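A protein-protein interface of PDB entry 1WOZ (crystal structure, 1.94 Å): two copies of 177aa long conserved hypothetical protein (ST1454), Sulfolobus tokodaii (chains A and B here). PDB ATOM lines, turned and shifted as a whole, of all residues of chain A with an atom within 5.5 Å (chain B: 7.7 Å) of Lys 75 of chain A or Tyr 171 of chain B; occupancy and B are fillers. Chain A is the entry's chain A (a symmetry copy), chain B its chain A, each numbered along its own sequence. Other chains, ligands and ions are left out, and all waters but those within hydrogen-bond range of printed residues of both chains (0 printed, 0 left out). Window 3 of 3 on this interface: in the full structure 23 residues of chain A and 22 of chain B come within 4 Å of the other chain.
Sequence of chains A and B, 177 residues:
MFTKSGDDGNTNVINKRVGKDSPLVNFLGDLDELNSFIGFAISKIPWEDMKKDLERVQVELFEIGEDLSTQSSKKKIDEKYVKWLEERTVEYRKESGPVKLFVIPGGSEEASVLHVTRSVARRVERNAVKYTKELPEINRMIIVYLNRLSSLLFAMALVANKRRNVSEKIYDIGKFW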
ATOM      1  N   VAL A  59     -22.520 -16.539  23.793  1.00  0.00           N
ATOM      2  CA  VAL A  59     -22.784 -15.154  24.167  1.00  0.00           C
ATOM      3  C   VAL A  59     -24.256 -15.055  24.595  1.00  0.00           C
ATOM      4  O   VAL A  59     -24.572 -14.450  25.632  1.00  0.00           O
ATOM      5  CB  VAL A  59     -22.535 -14.217  22.966  1.00  0.00           C
ATOM      6  CG1 VAL A  59     -23.092 -12.817  23.271  1.00  0.00           C
ATOM      7  CG2 VAL A  59     -21.028 -14.175  22.650  1.00  0.00           C
ATOM      8  N   PHE A  62     -25.122 -16.129  27.971  1.00  0.00           N
ATOM      9  CA  PHE A  62     -24.837 -15.105  28.991  1.00  0.00           C
ATOM     10  C   PHE A  62     -25.990 -14.097  28.986  1.00  0.00           C
ATOM     11  O   PHE A  62     -26.395 -13.600  30.031  1.00  0.00           O
ATOM     12  CB  PHE A  62     -23.512 -14.379  28.718  1.00  0.00           C
ATOM     13  CG  PHE A  62     -22.319 -15.066  29.322  1.00  0.00           C
ATOM     14  CD1 PHE A  62     -21.614 -16.030  28.616  1.00  0.00           C
ATOM     15  CD2 PHE A  62     -21.927 -14.776  30.633  1.00  0.00           C
ATOM     16  CE1 PHE A  62     -20.533 -16.705  29.205  1.00  0.00           C
ATOM     17  CE2 PHE A  62     -20.847 -15.449  31.220  1.00  0.00           C
ATOM     18  CZ  PHE A  62     -20.155 -16.417  30.492  1.00  0.00           C
ATOM     19  N   GLU A  63     -26.531 -13.786  27.808  1.00  0.00           N
ATOM     20  CA  GLU A  63     -27.660 -12.859  27.770  1.00  0.00           C
ATOM     21  C   GLU A  63     -28.879 -13.459  28.475  1.00  0.00           C
ATOM     22  O   GLU A  63     -29.637 -12.752  29.167  1.00  0.00           O
ATOM     23  CB  GLU A  63     -27.991 -12.490  26.322  1.00  0.00           C
ATOM     24  CG  GLU A  63     -26.875 -11.678  25.680  1.00  0.00           C
ATOM     25  CD  GLU A  63     -27.222 -11.142  24.298  1.00  0.00           C
ATOM     26  OE1 GLU A  63     -26.647 -10.108  23.920  1.00  0.00           O
ATOM     27  OE2 GLU A  63     -28.039 -11.753  23.581  1.00  0.00           O
ATOM     28  N   GLU A  66     -28.507 -12.982  32.088  1.00  0.00           N
ATOM     29  CA  GLU A  66     -28.792 -11.616  32.527  1.00  0.00           C
ATOM     30  C   GLU A  66     -30.291 -11.356  32.517  1.00  0.00           C
ATOM     31  O   GLU A  66     -30.811 -10.652  33.388  1.00  0.00           O
ATOM     32  CB  GLU A  66     -28.059 -10.600  31.639  1.00  0.00           C
ATOM     33  CG  GLU A  66     -26.552 -10.740  31.750  1.00  0.00           C
ATOM     34  CD  GLU A  66     -25.780  -9.466  31.429  1.00  0.00           C
ATOM     35  OE1 GLU A  66     -25.925  -8.911  30.316  1.00  0.00           O
ATOM     36  OE2 GLU A  66     -25.006  -9.044  32.312  1.00  0.00           O
ATOM     37  N   ASP A  67     -30.986 -11.923  31.537  1.00  0.00           N
ATOM     38  CA  ASP A  67     -32.440 -11.794  31.463  1.00  0.00           C
ATOM     39  C   ASP A  67     -32.970 -12.356  32.791  1.00  0.00           C
ATOM     40  O   ASP A  67     -33.654 -11.661  33.546  1.00  0.00           O
ATOM     41  CB  ASP A  67     -32.980 -12.609  30.264  1.00  0.00           C
ATOM     42  CG  ASP A  67     -34.483 -12.478  30.078  1.00  0.00           C
ATOM     43  OD1 ASP A  67     -35.220 -12.297  31.068  1.00  0.00           O
ATOM     44  OD2 ASP A  67     -34.936 -12.583  28.925  1.00  0.00           O
ATOM     45  N   THR A  70     -32.166 -10.305  36.018  1.00  0.00           N
ATOM     46  CA  THR A  70     -32.732  -8.958  36.112  1.00  0.00           C
ATOM     47  C   THR A  70     -34.204  -8.898  35.721  1.00  0.00           C
ATOM     48  O   THR A  70     -34.709  -7.823  35.389  1.00  0.00           O
ATOM     49  CB  THR A  70     -31.965  -7.962  35.208  1.00  0.00           C
ATOM     50  OG1 THR A  70     -32.196  -8.280  33.833  1.00  0.00           O
ATOM     51  CG2 THR A  70     -30.466  -8.035  35.484  1.00  0.00           C
ATOM     52  N   SER A  72     -35.710  -9.776  33.089  1.00  0.00           N
ATOM     53  CA  SER A  72     -35.793  -9.250  31.729  1.00  0.00           C
ATOM     54  C   SER A  72     -35.557  -7.738  31.595  1.00  0.00           C
ATOM     55  O   SER A  72     -35.945  -7.153  30.585  1.00  0.00           O
ATOM     56  CB  SER A  72     -37.152  -9.594  31.090  1.00  0.00           C
ATOM     57  OG  SER A  72     -37.474 -10.972  31.212  1.00  0.00           O
ATOM     58  N   SER A  73     -34.904  -7.123  32.583  1.00  0.00           N
ATOM     59  CA  SER A  73     -34.628  -5.676  32.546  1.00  0.00           C
ATOM     60  C   SER A  73     -33.402  -5.286  31.727  1.00  0.00           C
ATOM     61  O   SER A  73     -33.460  -4.343  30.943  1.00  0.00           O
ATOM     62  CB  SER A  73     -34.452  -5.121  33.969  1.00  0.00           C
ATOM     63  OG  SER A  73     -35.663  -5.215  34.695  1.00  0.00           O
ATOM     64  N   LYS A  74     -32.295  -6.004  31.917  1.00  0.00           N
ATOM     65  CA  LYS A  74     -31.043  -5.722  31.209  1.00  0.00           C
ATOM     66  C   LYS A  74     -30.929  -6.393  29.833  1.00  0.00           C
ATOM     67  O   LYS A  74     -30.237  -5.903  28.936  1.00  0.00           O
ATOM     68  CB  LYS A  74     -29.856  -6.143  32.064  1.00  0.00           C
ATOM     69  CG  LYS A  74     -28.519  -5.781  31.442  1.00  0.00           C
ATOM     70  CD  LYS A  74     -27.356  -6.182  32.318  1.00  0.00           C
ATOM     71  CE  LYS A  74     -26.034  -5.773  31.667  1.00  0.00           C
ATOM     72  NZ  LYS A  74     -24.888  -6.451  32.329  1.00  0.00           N
ATOM     73  N   LYS A  75     -31.588  -7.532  29.683  1.00  0.00           N
ATOM     74  CA  LYS A  75     -31.604  -8.267  28.422  1.00  0.00           C
ATOM     75  C   LYS A  75     -32.965  -8.944  28.397  1.00  0.00           C
ATOM     76  O   LYS A  75     -33.496  -9.320  29.448  1.00  0.00           O
ATOM     77  CB  LYS A  75     -30.509  -9.341  28.388  1.00  0.00           C
ATOM     78  CG  LYS A  75     -29.068  -8.832  28.358  1.00  0.00           C
ATOM     79  CD  LYS A  75     -28.689  -8.288  26.990  1.00  0.00           C
ATOM     80  CE  LYS A  75     -27.240  -7.852  26.979  1.00  0.00           C
ATOM     81  NZ  LYS A  75     -26.801  -7.520  25.602  1.00  0.00           N
ATOM     82  N   LYS A  76     -33.541  -9.081  27.205  1.00  0.00           N
ATOM     83  CA  LYS A  76     -34.824  -9.753  27.073  1.00  0.00           C
ATOM     84  C   LYS A  76     -34.830 -10.643  25.842  1.00  0.00           C
ATOM     85  O   LYS A  76     -34.827 -10.175  24.709  1.00  0.00           O
ATOM     86  CB  LYS A  76     -35.971  -8.752  26.980  1.00  0.00           C
ATOM     87  CG  LYS A  76     -37.335  -9.426  27.014  1.00  0.00           C
ATOM     88  CD  LYS A  76     -38.448  -8.404  26.915  1.00  0.00           C
ATOM     89  CE  LYS A  76     -39.820  -9.051  27.002  1.00  0.00           C
ATOM     90  NZ  LYS A  76     -40.887  -8.037  26.742  1.00  0.00           N
ATOM     91  N   ILE A  77     -34.821 -11.941  26.081  1.00  0.00           N
ATOM     92  CA  ILE A  77     -34.831 -12.908  25.000  1.00  0.00           C
ATOM     93  C   ILE A  77     -36.175 -12.813  24.294  1.00  0.00           C
ATOM     94  O   ILE A  77     -37.222 -12.837  24.943  1.00  0.00           O
ATOM     95  CB  ILE A  77     -34.618 -14.330  25.566  1.00  0.00           C
ATOM     96  CG1 ILE A  77     -33.319 -14.357  26.386  1.00  0.00           C
ATOM     97  CG2 ILE A  77     -34.591 -15.359  24.443  1.00  0.00           C
ATOM     98  CD1 ILE A  77     -32.075 -13.842  25.628  1.00  0.00           C
ATOM     99  N   TYR A  81     -34.143 -14.284  18.574  1.00  0.00           N
ATOM    100  CA  TYR A  81     -33.101 -15.188  19.057  1.00  0.00           C
ATOM    101  C   TYR A  81     -33.473 -16.593  18.599  1.00  0.00           C
ATOM    102  O   TYR A  81     -32.655 -17.329  18.049  1.00  0.00           O
ATOM    103  CB  TYR A  81     -33.069 -15.220  20.582  1.00  0.00           C
ATOM    104  CG  TYR A  81     -32.346 -14.086  21.259  1.00  0.00           C
ATOM    105  CD1 TYR A  81     -31.060 -14.268  21.785  1.00  0.00           C
ATOM    106  CD2 TYR A  81     -32.956 -12.846  21.418  1.00  0.00           C
ATOM    107  CE1 TYR A  81     -30.406 -13.238  22.459  1.00  0.00           C
ATOM    108  CE2 TYR A  81     -32.311 -11.813  22.088  1.00  0.00           C
ATOM    109  CZ  TYR A  81     -31.044 -12.019  22.606  1.00  0.00           C
ATOM    110  OH  TYR A  81     -30.441 -11.007  23.307  1.00  0.00           O
ATOM    111  N   LYS B 100     -10.359 -10.043  32.159  1.00  0.00           N
ATOM    112  CA  LYS B 100     -11.652  -9.375  32.241  1.00  0.00           C
ATOM    113  C   LYS B 100     -12.718 -10.438  32.519  1.00  0.00           C
ATOM    114  O   LYS B 100     -12.580 -11.594  32.081  1.00  0.00           O
ATOM    115  CB  LYS B 100     -12.006  -8.729  30.901  1.00  0.00           C
ATOM    116  CG  LYS B 100     -11.181  -7.496  30.518  1.00  0.00           C
ATOM    117  CD  LYS B 100     -11.592  -7.057  29.111  1.00  0.00           C
ATOM    118  CE  LYS B 100     -11.377  -5.568  28.881  1.00  0.00           C
ATOM    119  NZ  LYS B 100      -9.958  -5.218  29.078  1.00  0.00           N
ATOM    120  N   LEU B 101     -13.779 -10.035  33.217  1.00  0.00           N
ATOM    121  CA  LEU B 101     -14.908 -10.921  33.529  1.00  0.00           C
ATOM    122  C   LEU B 101     -16.116 -10.412  32.721  1.00  0.00           C
ATOM    123  O   LEU B 101     -16.223  -9.202  32.466  1.00  0.00           O
ATOM    124  CB  LEU B 101     -15.191 -10.863  35.039  1.00  0.00           C
ATOM    125  CG  LEU B 101     -13.973 -11.273  35.886  1.00  0.00           C
ATOM    126  CD1 LEU B 101     -14.285 -11.069  37.379  1.00  0.00           C
ATOM    127  CD2 LEU B 101     -13.621 -12.754  35.593  1.00  0.00           C
ATOM    128  N   PHE B 102     -17.011 -11.300  32.278  1.00  0.00           N
ATOM    129  CA  PHE B 102     -16.931 -12.746  32.493  1.00  0.00           C
ATOM    130  C   PHE B 102     -16.149 -13.426  31.385  1.00  0.00           C
ATOM    131  O   PHE B 102     -16.164 -12.978  30.250  1.00  0.00           O
ATOM    132  CB  PHE B 102     -18.328 -13.378  32.463  1.00  0.00           C
ATOM    133  CG  PHE B 102     -19.199 -13.002  33.603  1.00  0.00           C
ATOM    134  CD1 PHE B 102     -20.472 -12.493  33.373  1.00  0.00           C
ATOM    135  CD2 PHE B 102     -18.773 -13.188  34.912  1.00  0.00           C
ATOM    136  CE1 PHE B 102     -21.311 -12.175  34.439  1.00  0.00           C
ATOM    137  CE2 PHE B 102     -19.608 -12.870  35.984  1.00  0.00           C
ATOM    138  CZ  PHE B 102     -20.875 -12.364  35.745  1.00  0.00           C
ATOM    139  N   VAL B 103     -15.487 -14.528  31.722  1.00  0.00           N
ATOM    140  CA  VAL B 103     -14.768 -15.312  30.734  1.00  0.00           C
ATOM    141  C   VAL B 103     -15.788 -16.302  30.143  1.00  0.00           C
ATOM    142  O   VAL B 103     -16.512 -16.975  30.883  1.00  0.00           O
ATOM    143  CB  VAL B 103     -13.593 -16.096  31.387  1.00  0.00           C
ATOM    144  CG1 VAL B 103     -13.105 -17.214  30.446  1.00  0.00           C
ATOM    145  CG2 VAL B 103     -12.456 -15.125  31.698  1.00  0.00           C
ATOM    146  N   ILE B 104     -15.867 -16.359  28.815  1.00  0.00           N
ATOM    147  CA  ILE B 104     -16.769 -17.296  28.136  1.00  0.00           C
ATOM    148  C   ILE B 104     -15.979 -18.598  28.120  1.00  0.00           C
ATOM    149  O   ILE B 104     -14.891 -18.676  27.527  1.00  0.00           O
ATOM    150  CB  ILE B 104     -17.077 -16.825  26.701  1.00  0.00           C
ATOM    151  CG1 ILE B 104     -17.869 -15.502  26.767  1.00  0.00           C
ATOM    152  CG2 ILE B 104     -17.862 -17.935  25.941  1.00  0.00           C
ATOM    153  CD1 ILE B 104     -18.184 -14.864  25.385  1.00  0.00           C
ATOM    154  N   GLU B 168      -8.676 -15.247  25.519  1.00  0.00           N
ATOM    155  CA  GLU B 168      -9.916 -15.479  26.236  1.00  0.00           C
ATOM    156  C   GLU B 168     -11.043 -14.725  25.531  1.00  0.00           C
ATOM    157  O   GLU B 168     -10.840 -13.608  25.036  1.00  0.00           O
ATOM    158  CB  GLU B 168      -9.820 -14.941  27.662  1.00  0.00           C
ATOM    159  CG  GLU B 168      -8.748 -15.596  28.518  1.00  0.00           C
ATOM    160  CD  GLU B 168      -8.999 -17.074  28.715  1.00  0.00           C
ATOM    161  OE1 GLU B 168     -10.173 -17.485  28.635  1.00  0.00           O
ATOM    162  OE2 GLU B 168      -8.027 -17.812  28.966  1.00  0.00           O
ATOM    163  N   LYS B 169     -12.218 -15.340  25.476  1.00  0.00           N
ATOM    164  CA  LYS B 169     -13.398 -14.697  24.900  1.00  0.00           C
ATOM    165  C   LYS B 169     -14.090 -14.107  26.133  1.00  0.00           C
ATOM    166  O   LYS B 169     -14.216 -14.781  27.134  1.00  0.00           O
ATOM    167  CB  LYS B 169     -14.331 -15.725  24.260  1.00  0.00           C
ATOM    168  CG  LYS B 169     -13.651 -16.672  23.284  1.00  0.00           C
ATOM    169  CD  LYS B 169     -13.351 -16.010  21.964  1.00  0.00           C
ATOM    170  CE  LYS B 169     -12.879 -17.058  20.934  1.00  0.00           C
ATOM    171  NZ  LYS B 169     -12.819 -16.484  19.576  1.00  0.00           N
ATOM    172  N   ILE B 170     -14.535 -12.864  26.041  1.00  0.00           N
ATOM    173  CA  ILE B 170     -15.156 -12.159  27.160  1.00  0.00           C
ATOM    174  C   ILE B 170     -16.599 -11.658  26.908  1.00  0.00           C
ATOM    175  O   ILE B 170     -16.920 -11.154  25.824  1.00  0.00           O
ATOM    176  CB  ILE B 170     -14.310 -10.887  27.526  1.00  0.00           C
ATOM    177  CG1 ILE B 170     -12.800 -11.215  27.546  1.00  0.00           C
ATOM    178  CG2 ILE B 170     -14.775 -10.297  28.882  1.00  0.00           C
ATOM    179  CD1 ILE B 170     -12.349 -12.207  28.610  1.00  0.00           C
ATOM    180  N   TYR B 171     -17.451 -11.811  27.918  1.00  0.00           N
ATOM    181  CA  TYR B 171     -18.812 -11.281  27.897  1.00  0.00           C
ATOM    182  C   TYR B 171     -18.607 -10.268  29.024  1.00  0.00           C
ATOM    183  O   TYR B 171     -18.816 -10.552  30.209  1.00  0.00           O
ATOM    184  CB  TYR B 171     -19.844 -12.311  28.318  1.00  0.00           C
ATOM    185  CG  TYR B 171     -21.242 -11.729  28.282  1.00  0.00           C
ATOM    186  CD1 TYR B 171     -21.962 -11.664  27.082  1.00  0.00           C
ATOM    187  CD2 TYR B 171     -21.837 -11.214  29.443  1.00  0.00           C
ATOM    188  CE1 TYR B 171     -23.235 -11.107  27.039  1.00  0.00           C
ATOM    189  CE2 TYR B 171     -23.122 -10.648  29.410  1.00  0.00           C
ATOM    190  CZ  TYR B 171     -23.810 -10.606  28.208  1.00  0.00           C
ATOM    191  OH  TYR B 171     -25.088 -10.120  28.181  1.00  0.00           O
ATOM    192  N   ASP B 172     -18.164  -9.089  28.616  1.00  0.00           N
ATOM    193  CA  ASP B 172     -17.771  -8.015  29.509  1.00  0.00           C
ATOM    194  C   ASP B 172     -18.768  -7.394  30.471  1.00  0.00           C
ATOM    195  O   ASP B 172     -19.724  -6.737  30.047  1.00  0.00           O
ATOM    196  CB  ASP B 172     -17.134  -6.912  28.664  1.00  0.00           C
ATOM    197  CG  ASP B 172     -16.034  -6.204  29.394  1.00  0.00           C
ATOM    198  OD1 ASP B 172     -16.244  -5.879  30.579  1.00  0.00           O
ATOM    199  OD2 ASP B 172     -14.964  -5.981  28.778  1.00  0.00           O
ATOM    200  N   ILE B 173     -18.517  -7.562  31.764  1.00  0.00           N
ATOM    201  CA  ILE B 173     -19.400  -6.991  32.787  1.00  0.00           C
ATOM    202  C   ILE B 173     -18.725  -5.822  33.508  1.00  0.00           C
ATOM    203  O   ILE B 173     -19.248  -5.311  34.490  1.00  0.00           O
ATOM    204  CB  ILE B 173     -19.832  -8.043  33.838  1.00  0.00           C
ATOM    205  CG1 ILE B 173     -18.599  -8.639  34.526  1.00  0.00           C
ATOM    206  CG2 ILE B 173     -20.672  -9.095  33.177  1.00  0.00           C
ATOM    207  CD1 ILE B 173     -18.894  -9.367  35.796  1.00  0.00           C
ATOM    208  N   GLY B 174     -17.551  -5.419  33.029  1.00  0.00           N
ATOM    209  CA  GLY B 174     -16.870  -4.277  33.613  1.00  0.00           C
ATOM    210  C   GLY B 174     -15.917  -4.492  34.766  1.00  0.00           C
ATOM    211  O   GLY B 174     -15.380  -3.523  35.312  1.00  0.00           O
ATOM    212  N   LYS B 175     -15.689  -5.747  35.140  1.00  0.00           N
ATOM    213  CA  LYS B 175     -14.776  -6.053  36.244  1.00  0.00           C
ATOM    214  C   LYS B 175     -13.661  -6.959  35.732  1.00  0.00           C
ATOM    215  O   LYS B 175     -13.821  -7.591  34.694  1.00  0.00           O
ATOM    216  CB  LYS B 175     -15.536  -6.808  37.349  1.00  0.00           C
ATOM    217  CG  LYS B 175     -16.675  -6.018  37.995  1.00  0.00           C
ATOM    218  CD  LYS B 175     -16.117  -4.934  38.896  1.00  0.00           C
ATOM    219  CE  LYS B 175     -15.221  -5.551  39.979  1.00  0.00           C
ATOM    220  NZ  LYS B 175     -14.686  -4.531  40.909  1.00  0.00           N
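OE1 of Glu 66 of chain A sits at hydrogen-bond distance from OH of Tyr 171 of chain B (2.6 Å).
Printed residues of chain B within 4 Å of Val 59 of chain A: Tyr 171 (3.9 Å).
Printed residues of chain B within 4 Å of Glu 63 of chain A: Tyr 171.
Printed residues of chain B within 4 Å of Glu 66 of chain A: Tyr 171 (2.6 Å).
Ser 72 of chain A touches none of the printed residues of chain B.
Printed residues of chain A within 4 Å of Phe 102 of chain B: Phe 62.
Of the printed residues of chain A, Val 103 of chain B touches Phe 62.
Of chain A, only Val 59, Phe 62, Glu 63, Glu 66 and Lys 75 come within 4 Å of Tyr 171 of chain B.
The nearest printed residue of chain B that does not touch Lys 75 of chain A is Asp 172 of chain B (8.2 Å).
The nearest printed residue of chain A that does not touch Ile 104 of chain B is Val 59 of chain A (4.01 Å).
Among the printed residues, pairs that only touch across the chains: Lys 75 of chain A with Tyr 171 of chain B (3.3 Å), Glu 63 of chain A with Tyr 171 of chain B (3.4 Å), Phe 62 of chain A with Phe 102 of chain B (3.5 Å), Phe 62 of chain A with Tyr 171 of chain B (3.5 Å), Phe 62 of chain A with Val 103 of chain B (3.7 Å), Phe 62 of chain A with Ile 104 of chain B (3.8 Å) and Val 59 of chain A with Tyr 171 of chain B (3.9 Å).
No position is printed for both chains.
N of Phe 102 of chain B lies within hydrogen-bond range of O of Tyr 171 of chain B, 2.8 Å away.
The backbone carbonyl oxygen (O) of Lys 169 of chain B lies within hydrogen-bond range of the backbone NH (N) of Ile 104 of chain B.
The side-chain carboxylate of Glu 63 of chain A lies within salt-bridge range of the side-chain amino group of Lys 75 of chain A.
The side-chain hydroxyl (OH) of Tyr 81 of chain A sits at hydrogen-bond distance from the side-chain carboxylate (OE2) of Glu 63 of chain A, at 2.5 Å.
The side-chain hydroxyl (OG1) of Thr 70 of chain A is in hydrogen-bond range of the backbone carbonyl oxygen (O) of Glu 66 of chain A (2.8 Å).
The side-chain carboxylate (OE2) of Glu 66 of chain A lies within salt-bridge range of the side-chain amino group (NZ) of Lys 74 of chain A (2.6 Å).
Of the 13 printed residues of chain A, 5 touch a printed residue of chain B.
Hydrophobic or aromatic side chains of chain A that line the printed part of chain B: Phe 62.
Along chain A the printed residues that touch a printed residue of chain B span positions 59 to 75.
Hydrophobic or aromatic side chains of chain B that line the printed part of chain A: Phe 102, Ile 104 and Tyr 171.
Among the printed residues, 8 pairs touch across the chains.
Among the printed residues, no Asp or Glu carboxylate lies within 4 Å of a Lys or Arg side-chain nitrogen of the other chain.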
